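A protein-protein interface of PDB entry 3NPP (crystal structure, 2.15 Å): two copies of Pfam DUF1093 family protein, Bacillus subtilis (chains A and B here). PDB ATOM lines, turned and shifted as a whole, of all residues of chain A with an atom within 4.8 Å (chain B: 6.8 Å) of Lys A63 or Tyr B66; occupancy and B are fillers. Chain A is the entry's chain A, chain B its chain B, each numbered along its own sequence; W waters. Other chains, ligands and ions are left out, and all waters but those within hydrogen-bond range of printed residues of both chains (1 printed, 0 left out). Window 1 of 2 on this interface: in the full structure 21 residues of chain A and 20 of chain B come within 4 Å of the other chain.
O of Phe A3 sits at hydrogen-bond distance from N of Thr B45 (3.0 Å). The backbone NH of Asn A4 sits at hydrogen-bond distance from the backbone carbonyl oxygen of Lys B65 (2.9 Å). The backbone NH of Val B67 is in hydrogen-bond range of the backbone carbonyl oxygen of Asn A4. The backbone NH of His A8 lies within hydrogen-bond range of the side-chain hydroxyl of Tyr B66, at 3.1 Å.
The side-chain amide oxygen (OD1) of Asn A4 is in hydrogen-bond range of the backbone NH (N) of Phe A6, at 2.8 Å. The backbone carbonyl oxygen (O) of His A8 lies within hydrogen-bond range of the backbone NH (N) of Gly A64, at 2.9 Å. NZ of Lys A63 lies within salt-bridge range of OE1 of Glu A68, at 2.7 Å. NZ of Lys B63 is in salt-bridge range of OE2 of Glu B68 (3.3 Å).
Among the printed residues, merely in contact across the chains: Phe A3 with Gly B64 (3.1 Å), Phe A6 with Tyr B66 (3.2 Å), Asn A4 with Tyr B66 (3.3 Å), Phe A3 with Lys B65 (3.3 Å), Gly A64 with Phe B3 (3.3 Å), Lys A65 with Phe B3 (3.3 Å), Ile A7 with Tyr B66 (3.3 Å), Tyr A66 with Ile B7 (3.4 Å), Gly A64 with Tyr B66 (3.4 Å), Phe A3 with Ala B62 (3.5 Å), Ala A62 with Phe B3 (3.5 Å), Asn A4 with Thr B45 (3.8 Å), Phe A3 with Val B67 (3.9 Å), Lys A63 with Tyr B66 (3.9 Å) and Tyr A66 with Lys B63 (3.9 Å).
Of chain B, only Tyr B66 (3.9 Å) comes within 4 Å of Lys A63. Printed residues of chain A within 4 Å of Phe B3: Ala A62, Gly A64 and Lys A65. Of the printed residues of chain B, Phe A3 touches Thr B45, Ala B62, Gly B64, Lys B65 and Val B67. Printed residues of chain A within 4 Å of Thr B45: Phe A3 and Asn A4. Of the printed residues of chain B, Phe A6 touches Tyr B66. Printed residues of chain B within 4 Å of Gly A64: Phe B3 and Tyr B66.
Of the 13 printed residues of chain B, 9 touch a printed residue of chain A. Hydrophobic or aromatic side chains of chain B that line the printed part of chain A: Phe B3, Ile B7, Ala B62, Tyr B66 and Val B67. Of the 13 printed residues of chain A, 10 touch a printed residue of chain B. Among the printed residues, 19 pairs touch across the chains. Among the printed residues, no Asp or Glu carboxylate lies within 4 Å of a Lys or Arg side-chain nitrogen of the other chain.
Phe A3 touches Ala B62, and with the chains exchanged Ala A62 touches Phe B3. Phe A3 touches Gly B64, and with the chains exchanged Gly A64 touches Phe B3. Phe A3 touches Lys B65, and with the chains exchanged Lys A65 touches Phe B3. Gly A64 touches Tyr B66, but with the chains exchanged Tyr A66 does not touch Gly B64 (6.9 Å). Of the 19 pairs that touch across the chains among the printed residues, 10 have their exchanged pair printed and touching as well.
Water W1 lies within hydrogen-bond range of the side-chain hydroxyl (OG1) of Thr B45 and the backbone carbonyl oxygen (O) of Phe A3.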
ATOM      1  N   PHE A   3     -14.149  -7.579  11.514  1.00  0.00           N
ATOM      2  CA  PHE A   3     -15.294  -8.237  12.146  1.00  0.00           C
ATOM      3  C   PHE A   3     -16.555  -7.439  11.925  1.00  0.00           C
ATOM      4  O   PHE A   3     -16.505  -6.231  11.949  1.00  0.00           O
ATOM      5  CB  PHE A   3     -15.034  -8.438  13.640  1.00  0.00           C
ATOM      6  CG  PHE A   3     -13.736  -9.172  13.927  1.00  0.00           C
ATOM      7  CD1 PHE A   3     -12.561  -8.502  13.939  1.00  0.00           C
ATOM      8  CD2 PHE A   3     -13.709 -10.538  14.119  1.00  0.00           C
ATOM      9  CE1 PHE A   3     -11.359  -9.169  14.159  1.00  0.00           C
ATOM     10  CE2 PHE A   3     -12.479 -11.192  14.361  1.00  0.00           C
ATOM     11  CZ  PHE A   3     -11.344 -10.512  14.366  1.00  0.00           C
ATOM     12  N   ASN A   4     -17.685  -8.152  11.712  1.00  0.00           N
ATOM     13  CA  ASN A   4     -18.976  -7.546  11.375  1.00  0.00           C
ATOM     14  C   ASN A   4     -20.143  -8.110  12.241  1.00  0.00           C
ATOM     15  O   ASN A   4     -20.027  -9.201  12.821  1.00  0.00           O
ATOM     16  CB  ASN A   4     -19.244  -7.683   9.866  1.00  0.00           C
ATOM     17  CG  ASN A   4     -19.647  -9.076   9.465  1.00  0.00           C
ATOM     18  OD1 ASN A   4     -20.791  -9.485   9.666  1.00  0.00           O
ATOM     19  ND2 ASN A   4     -18.720  -9.809   8.848  1.00  0.00           N
ATOM     20  N   PHE A   6     -23.194  -8.927  11.002  1.00  0.00           N
ATOM     21  CA  PHE A   6     -24.256  -9.355  10.036  1.00  0.00           C
ATOM     22  C   PHE A   6     -24.401 -10.868  10.136  1.00  0.00           C
ATOM     23  O   PHE A   6     -23.811 -11.615   9.365  1.00  0.00           O
ATOM     24  CB  PHE A   6     -23.962  -8.893   8.610  1.00  0.00           C
ATOM     25  CG  PHE A   6     -23.493  -7.450   8.506  1.00  0.00           C
ATOM     26  CD1 PHE A   6     -24.219  -6.418   9.097  1.00  0.00           C
ATOM     27  CD2 PHE A   6     -22.348  -7.122   7.799  1.00  0.00           C
ATOM     28  CE1 PHE A   6     -23.798  -5.100   8.992  1.00  0.00           C
ATOM     29  CE2 PHE A   6     -21.913  -5.794   7.702  1.00  0.00           C
ATOM     30  CZ  PHE A   6     -22.643  -4.790   8.289  1.00  0.00           C
ATOM     31  N   ILE A   7     -25.147 -11.312  11.153  1.00  0.00           N
ATOM     32  CA  ILE A   7     -25.142 -12.731  11.585  1.00  0.00           C
ATOM     33  C   ILE A   7     -26.083 -13.588  10.714  1.00  0.00           C
ATOM     34  O   ILE A   7     -27.281 -13.377  10.699  1.00  0.00           O
ATOM     35  CB  ILE A   7     -25.535 -12.930  13.099  1.00  0.00           C
ATOM     36  CG1 ILE A   7     -24.783 -11.963  14.037  1.00  0.00           C
ATOM     37  CG2 ILE A   7     -25.255 -14.403  13.532  1.00  0.00           C
ATOM     38  CD1 ILE A   7     -23.259 -12.026  13.927  1.00  0.00           C
ATOM     39  N   HIS A   8     -25.510 -14.572  10.023  1.00  0.00           N
ATOM     40  CA  HIS A   8     -26.218 -15.437   9.095  1.00  0.00           C
ATOM     41  C   HIS A   8     -26.411 -16.786   9.788  1.00  0.00           C
ATOM     42  O   HIS A   8     -25.458 -17.470  10.058  1.00  0.00           O
ATOM     43  CB  HIS A   8     -25.381 -15.608   7.804  1.00  0.00           C
ATOM     44  CG  HIS A   8     -25.992 -16.539   6.788  1.00  0.00           C
ATOM     45  ND1 HIS A   8     -25.293 -16.988   5.681  1.00  0.00           N
ATOM     46  CD2 HIS A   8     -27.241 -17.049   6.672  1.00  0.00           C
ATOM     47  CE1 HIS A   8     -26.077 -17.778   4.964  1.00  0.00           C
ATOM     48  NE2 HIS A   8     -27.265 -17.828   5.545  1.00  0.00           N
ATOM     49  N   GLN A   9     -27.650 -17.154  10.059  1.00  0.00           N
ATOM     50  CA  GLN A   9     -27.959 -18.456  10.662  1.00  0.00           C
ATOM     51  C   GLN A   9     -28.193 -19.470   9.543  1.00  0.00           C
ATOM     52  O   GLN A   9     -28.890 -19.175   8.574  1.00  0.00           O
ATOM     53  CB  GLN A   9     -29.207 -18.364  11.530  1.00  0.00           C
ATOM     54  CG  GLN A   9     -29.657 -19.739  12.149  1.00  0.00           C
ATOM     55  CD  GLN A   9     -30.678 -19.591  13.271  1.00  0.00           C
ATOM     56  OE1 GLN A   9     -30.569 -18.702  14.099  1.00  0.00           O
ATOM     57  NE2 GLN A   9     -31.669 -20.491  13.306  1.00  0.00           N
ATOM     58  N   LYS A  61     -27.718 -26.410  14.087  1.00  0.00           N
ATOM     59  CA  LYS A  61     -27.857 -24.969  13.898  1.00  0.00           C
ATOM     60  C   LYS A  61     -26.474 -24.344  13.933  1.00  0.00           C
ATOM     61  O   LYS A  61     -25.659 -24.666  14.827  1.00  0.00           O
ATOM     62  CB  LYS A  61     -28.731 -24.388  14.981  1.00  0.00           C
ATOM     63  CG  LYS A  61     -28.983 -22.891  14.865  1.00  0.00           C
ATOM     64  CD  LYS A  61     -29.913 -22.380  15.922  1.00  0.00           C
ATOM     65  CE  LYS A  61     -29.272 -22.290  17.300  1.00  0.00           C
ATOM     66  NZ  LYS A  61     -30.284 -21.973  18.354  1.00  0.00           N
ATOM     67  N   ALA A  62     -26.216 -23.451  12.973  1.00  0.00           N
ATOM     68  CA  ALA A  62     -24.948 -22.797  12.822  1.00  0.00           C
ATOM     69  C   ALA A  62     -25.160 -21.313  12.715  1.00  0.00           C
ATOM     70  O   ALA A  62     -26.227 -20.853  12.298  1.00  0.00           O
ATOM     71  CB  ALA A  62     -24.212 -23.323  11.588  1.00  0.00           C
ATOM     72  N   LYS A  63     -24.158 -20.562  13.150  1.00  0.00           N
ATOM     73  CA  LYS A  63     -24.049 -19.114  12.904  1.00  0.00           C
ATOM     74  C   LYS A  63     -22.771 -18.940  12.134  1.00  0.00           C
ATOM     75  O   LYS A  63     -21.708 -19.365  12.611  1.00  0.00           O
ATOM     76  CB  LYS A  63     -23.960 -18.334  14.216  1.00  0.00           C
ATOM     77  CG  LYS A  63     -25.019 -18.658  15.236  1.00  0.00           C
ATOM     78  CD  LYS A  63     -26.425 -18.291  14.817  1.00  0.00           C
ATOM     79  CE  LYS A  63     -27.454 -18.800  15.865  1.00  0.00           C
ATOM     80  NZ  LYS A  63     -27.210 -18.177  17.229  1.00  0.00           N
ATOM     81  N   GLY A  64     -22.849 -18.329  10.964  1.00  0.00           N
ATOM     82  CA  GLY A  64     -21.738 -18.349  10.008  1.00  0.00           C
ATOM     83  C   GLY A  64     -21.399 -19.807   9.697  1.00  0.00           C
ATOM     84  O   GLY A  64     -22.305 -20.607   9.409  1.00  0.00           O
ATOM     85  N   LYS A  65     -20.127 -20.169   9.856  1.00  0.00           N
ATOM     86  CA  LYS A  65     -19.682 -21.554   9.678  1.00  0.00           C
ATOM     87  C   LYS A  65     -19.553 -22.344  10.994  1.00  0.00           C
ATOM     88  O   LYS A  65     -19.131 -23.507  10.959  1.00  0.00           O
ATOM     89  CB  LYS A  65     -18.366 -21.608   8.875  1.00  0.00           C
ATOM     90  CG  LYS A  65     -17.139 -21.263   9.655  1.00  0.00           C
ATOM     91  N   TYR A  66     -20.001 -21.757  12.115  1.00  0.00           N
ATOM     92  CA  TYR A  66     -19.801 -22.319  13.453  1.00  0.00           C
ATOM     93  C   TYR A  66     -21.094 -23.004  13.913  1.00  0.00           C
ATOM     94  O   TYR A  66     -22.113 -22.357  14.076  1.00  0.00           O
ATOM     95  CB  TYR A  66     -19.372 -21.212  14.419  1.00  0.00           C
ATOM     96  CG  TYR A  66     -19.378 -21.549  15.913  1.00  0.00           C
ATOM     97  CD1 TYR A  66     -18.404 -22.404  16.456  1.00  0.00           C
ATOM     98  CD2 TYR A  66     -20.280 -20.905  16.821  1.00  0.00           C
ATOM     99  CE1 TYR A  66     -18.330 -22.676  17.842  1.00  0.00           C
ATOM    100  CE2 TYR A  66     -20.223 -21.193  18.240  1.00  0.00           C
ATOM    101  CZ  TYR A  66     -19.244 -22.104  18.723  1.00  0.00           C
ATOM    102  OH  TYR A  66     -19.125 -22.420  20.078  1.00  0.00           O
ATOM    103  N   GLU A  68     -23.553 -24.593  16.579  1.00  0.00           N
ATOM    104  CA  GLU A  68     -23.905 -24.275  17.964  1.00  0.00           C
ATOM    105  C   GLU A  68     -24.655 -25.348  18.701  1.00  0.00           C
ATOM    106  O   GLU A  68     -24.362 -25.591  19.866  1.00  0.00           O
ATOM    107  CB  GLU A  68     -24.722 -23.012  17.986  1.00  0.00           C
ATOM    108  CG  GLU A  68     -23.953 -21.839  17.450  1.00  0.00           C
ATOM    109  CD  GLU A  68     -24.434 -20.518  17.990  1.00  0.00           C
ATOM    110  OE1 GLU A  68     -25.662 -20.291  17.969  1.00  0.00           O
ATOM    111  OE2 GLU A  68     -23.582 -19.686  18.357  1.00  0.00           O
ATOM    112  N   PHE B   3     -19.125 -26.877   7.913  1.00  0.00           N
ATOM    113  CA  PHE B   3     -19.453 -26.337   9.222  1.00  0.00           C
ATOM    114  C   PHE B   3     -18.753 -27.183  10.274  1.00  0.00           C
ATOM    115  O   PHE B   3     -18.605 -28.395  10.105  1.00  0.00           O
ATOM    116  CB  PHE B   3     -20.967 -26.367   9.460  1.00  0.00           C
ATOM    117  CG  PHE B   3     -21.749 -25.523   8.490  1.00  0.00           C
ATOM    118  CD1 PHE B   3     -22.014 -25.984   7.219  1.00  0.00           C
ATOM    119  CD2 PHE B   3     -22.186 -24.253   8.834  1.00  0.00           C
ATOM    120  CE1 PHE B   3     -22.704 -25.205   6.313  1.00  0.00           C
ATOM    121  CE2 PHE B   3     -22.867 -23.459   7.905  1.00  0.00           C
ATOM    122  CZ  PHE B   3     -23.134 -23.947   6.652  1.00  0.00           C
ATOM    123  N   ILE B   7     -14.379 -22.636  16.197  1.00  0.00           N
ATOM    124  CA  ILE B   7     -14.291 -21.228  15.821  1.00  0.00           C
ATOM    125  C   ILE B   7     -13.280 -20.469  16.655  1.00  0.00           C
ATOM    126  O   ILE B   7     -13.124 -20.710  17.867  1.00  0.00           O
ATOM    127  CB  ILE B   7     -15.647 -20.535  15.882  1.00  0.00           C
ATOM    128  CG1 ILE B   7     -15.690 -19.335  14.906  1.00  0.00           C
ATOM    129  CG2 ILE B   7     -16.022 -20.193  17.379  1.00  0.00           C
ATOM    130  CD1 ILE B   7     -15.464 -19.738  13.360  1.00  0.00           C
ATOM    131  N   THR B  45     -16.969  -3.702  13.398  1.00  0.00           N
ATOM    132  CA  THR B  45     -18.166  -2.939  13.069  1.00  0.00           C
ATOM    133  C   THR B  45     -19.287  -3.510  13.919  1.00  0.00           C
ATOM    134  O   THR B  45     -19.506  -4.730  13.934  1.00  0.00           O
ATOM    135  CB  THR B  45     -18.510  -3.028  11.562  1.00  0.00           C
ATOM    136  OG1 THR B  45     -17.530  -2.302  10.830  1.00  0.00           O
ATOM    137  CG2 THR B  45     -19.897  -2.452  11.262  1.00  0.00           C
ATOM    138  N   VAL B  60     -14.591  -6.202  22.989  1.00  0.00           N
ATOM    139  CA  VAL B  60     -15.529  -6.839  22.035  1.00  0.00           C
ATOM    140  C   VAL B  60     -15.167  -8.323  21.912  1.00  0.00           C
ATOM    141  O   VAL B  60     -14.019  -8.639  21.654  1.00  0.00           O
ATOM    142  CB  VAL B  60     -15.418  -6.194  20.622  1.00  0.00           C
ATOM    143  CG1 VAL B  60     -16.482  -6.757  19.688  1.00  0.00           C
ATOM    144  CG2 VAL B  60     -15.546  -4.669  20.693  1.00  0.00           C
ATOM    145  N   LYS B  61     -16.131  -9.231  22.106  1.00  0.00           N
ATOM    146  CA  LYS B  61     -15.875 -10.654  21.872  1.00  0.00           C
ATOM    147  C   LYS B  61     -16.157 -10.958  20.413  1.00  0.00           C
ATOM    148  O   LYS B  61     -17.270 -10.791  19.973  1.00  0.00           O
ATOM    149  CB  LYS B  61     -16.729 -11.556  22.762  1.00  0.00           C
ATOM    150  CG  LYS B  61     -16.259 -13.066  22.693  1.00  0.00           C
ATOM    151  CD  LYS B  61     -17.112 -14.009  23.546  1.00  0.00           C
ATOM    152  CE  LYS B  61     -16.919 -13.737  25.049  1.00  0.00           C
ATOM    153  NZ  LYS B  61     -17.780 -14.628  25.835  1.00  0.00           N
ATOM    154  N   ALA B  62     -15.126 -11.396  19.691  1.00  0.00           N
ATOM    155  CA  ALA B  62     -15.204 -11.759  18.293  1.00  0.00           C
ATOM    156  C   ALA B  62     -15.190 -13.272  18.203  1.00  0.00           C
ATOM    157  O   ALA B  62     -14.394 -13.909  18.864  1.00  0.00           O
ATOM    158  CB  ALA B  62     -14.033 -11.188  17.529  1.00  0.00           C
ATOM    159  N   LYS B  63     -16.076 -13.824  17.375  1.00  0.00           N
ATOM    160  CA  LYS B  63     -16.228 -15.255  17.173  1.00  0.00           C
ATOM    161  C   LYS B  63     -16.193 -15.399  15.629  1.00  0.00           C
ATOM    162  O   LYS B  63     -17.138 -14.982  14.922  1.00  0.00           O
ATOM    163  CB  LYS B  63     -17.578 -15.681  17.799  1.00  0.00           C
ATOM    164  CG  LYS B  63     -17.834 -17.184  18.029  1.00  0.00           C
ATOM    165  CD  LYS B  63     -17.502 -17.648  19.519  1.00  0.00           C
ATOM    166  CE  LYS B  63     -18.763 -18.186  20.302  1.00  0.00           C
ATOM    167  NZ  LYS B  63     -18.484 -18.326  21.808  1.00  0.00           N
ATOM    168  N   GLY B  64     -15.075 -15.920  15.115  1.00  0.00           N
ATOM    169  CA  GLY B  64     -14.825 -16.000  13.676  1.00  0.00           C
ATOM    170  C   GLY B  64     -14.728 -14.595  13.117  1.00  0.00           C
ATOM    171  O   GLY B  64     -14.118 -13.746  13.726  1.00  0.00           O
ATOM    172  N   LYS B  65     -15.459 -14.324  12.040  1.00  0.00           N
ATOM    173  CA  LYS B  65     -15.629 -12.952  11.513  1.00  0.00           C
ATOM    174  C   LYS B  65     -16.736 -12.114  12.210  1.00  0.00           C
ATOM    175  O   LYS B  65     -16.991 -10.999  11.778  1.00  0.00           O
ATOM    176  CB  LYS B  65     -15.871 -12.991   9.984  1.00  0.00           C
ATOM    177  CG  LYS B  65     -17.131 -13.799   9.519  1.00  0.00           C
ATOM    178  CD  LYS B  65     -17.518 -13.483   8.076  1.00  0.00           C
ATOM    179  CE  LYS B  65     -18.443 -14.516   7.522  1.00  0.00           C
ATOM    180  NZ  LYS B  65     -18.632 -14.328   6.061  1.00  0.00           N
ATOM    181  N   TYR B  66     -17.391 -12.621  13.266  1.00  0.00           N
ATOM    182  CA  TYR B  66     -18.545 -11.919  13.849  1.00  0.00           C
ATOM    183  C   TYR B  66     -18.226 -11.229  15.163  1.00  0.00           C
ATOM    184  O   TYR B  66     -17.534 -11.773  16.005  1.00  0.00           O
ATOM    185  CB  TYR B  66     -19.725 -12.847  14.077  1.00  0.00           C
ATOM    186  CG  TYR B  66     -20.429 -13.419  12.830  1.00  0.00           C
ATOM    187  CD1 TYR B  66     -20.585 -12.674  11.650  1.00  0.00           C
ATOM    188  CD2 TYR B  66     -21.021 -14.672  12.885  1.00  0.00           C
ATOM    189  CE1 TYR B  66     -21.240 -13.195  10.551  1.00  0.00           C
ATOM    190  CE2 TYR B  66     -21.693 -15.192  11.803  1.00  0.00           C
ATOM    191  CZ  TYR B  66     -21.810 -14.439  10.627  1.00  0.00           C
ATOM    192  OH  TYR B  66     -22.473 -14.924   9.526  1.00  0.00           O
ATOM    193  N   VAL B  67     -18.777 -10.032  15.331  1.00  0.00           N
ATOM    194  CA  VAL B  67     -18.903  -9.422  16.612  1.00  0.00           C
ATOM    195  C   VAL B  67     -20.073 -10.112  17.303  1.00  0.00           C
ATOM    196  O   VAL B  67     -21.160 -10.104  16.798  1.00  0.00           O
ATOM    197  CB  VAL B  67     -19.161  -7.923  16.511  1.00  0.00           C
ATOM    198  CG1 VAL B  67     -19.417  -7.343  17.888  1.00  0.00           C
ATOM    199  CG2 VAL B  67     -18.002  -7.247  15.854  1.00  0.00           C
ATOM    200  N   GLU B  68     -19.800 -10.702  18.462  1.00  0.00           N
ATOM    201  CA  GLU B  68     -20.762 -11.458  19.247  1.00  0.00           C
ATOM    202  C   GLU B  68     -21.372 -10.558  20.299  1.00  0.00           C
ATOM    203  O   GLU B  68     -22.580 -10.463  20.415  1.00  0.00           O
ATOM    204  CB  GLU B  68     -20.063 -12.660  19.902  1.00  0.00           C
ATOM    205  CG  GLU B  68     -20.854 -13.368  20.966  1.00  0.00           C
ATOM    206  CD  GLU B  68     -20.574 -14.835  20.987  1.00  0.00           C
ATOM    207  OE1 GLU B  68     -21.159 -15.535  20.123  1.00  0.00           O
ATOM    208  OE2 GLU B  68     -19.792 -15.282  21.836  1.00  0.00           O
ATOM    209  N   THR B  69     -20.530  -9.935  21.090  1.00  0.00           N
ATOM    210  CA  THR B  69     -21.000  -9.001  22.099  1.00  0.00           C
ATOM    211  C   THR B  69     -19.871  -8.058  22.496  1.00  0.00           C
ATOM    212  O   THR B  69     -18.749  -8.213  22.041  1.00  0.00           O
ATOM    213  CB  THR B  69     -21.571  -9.756  23.352  1.00  0.00           C
ATOM    214  OG1 THR B  69     -22.242  -8.810  24.198  1.00  0.00           O
ATOM    215  CG2 THR B  69     -20.459 -10.511  24.121  1.00  0.00           C
HETATM  216  O   HOH W   1     -15.880  -4.237  10.144  1.00  0.00           O
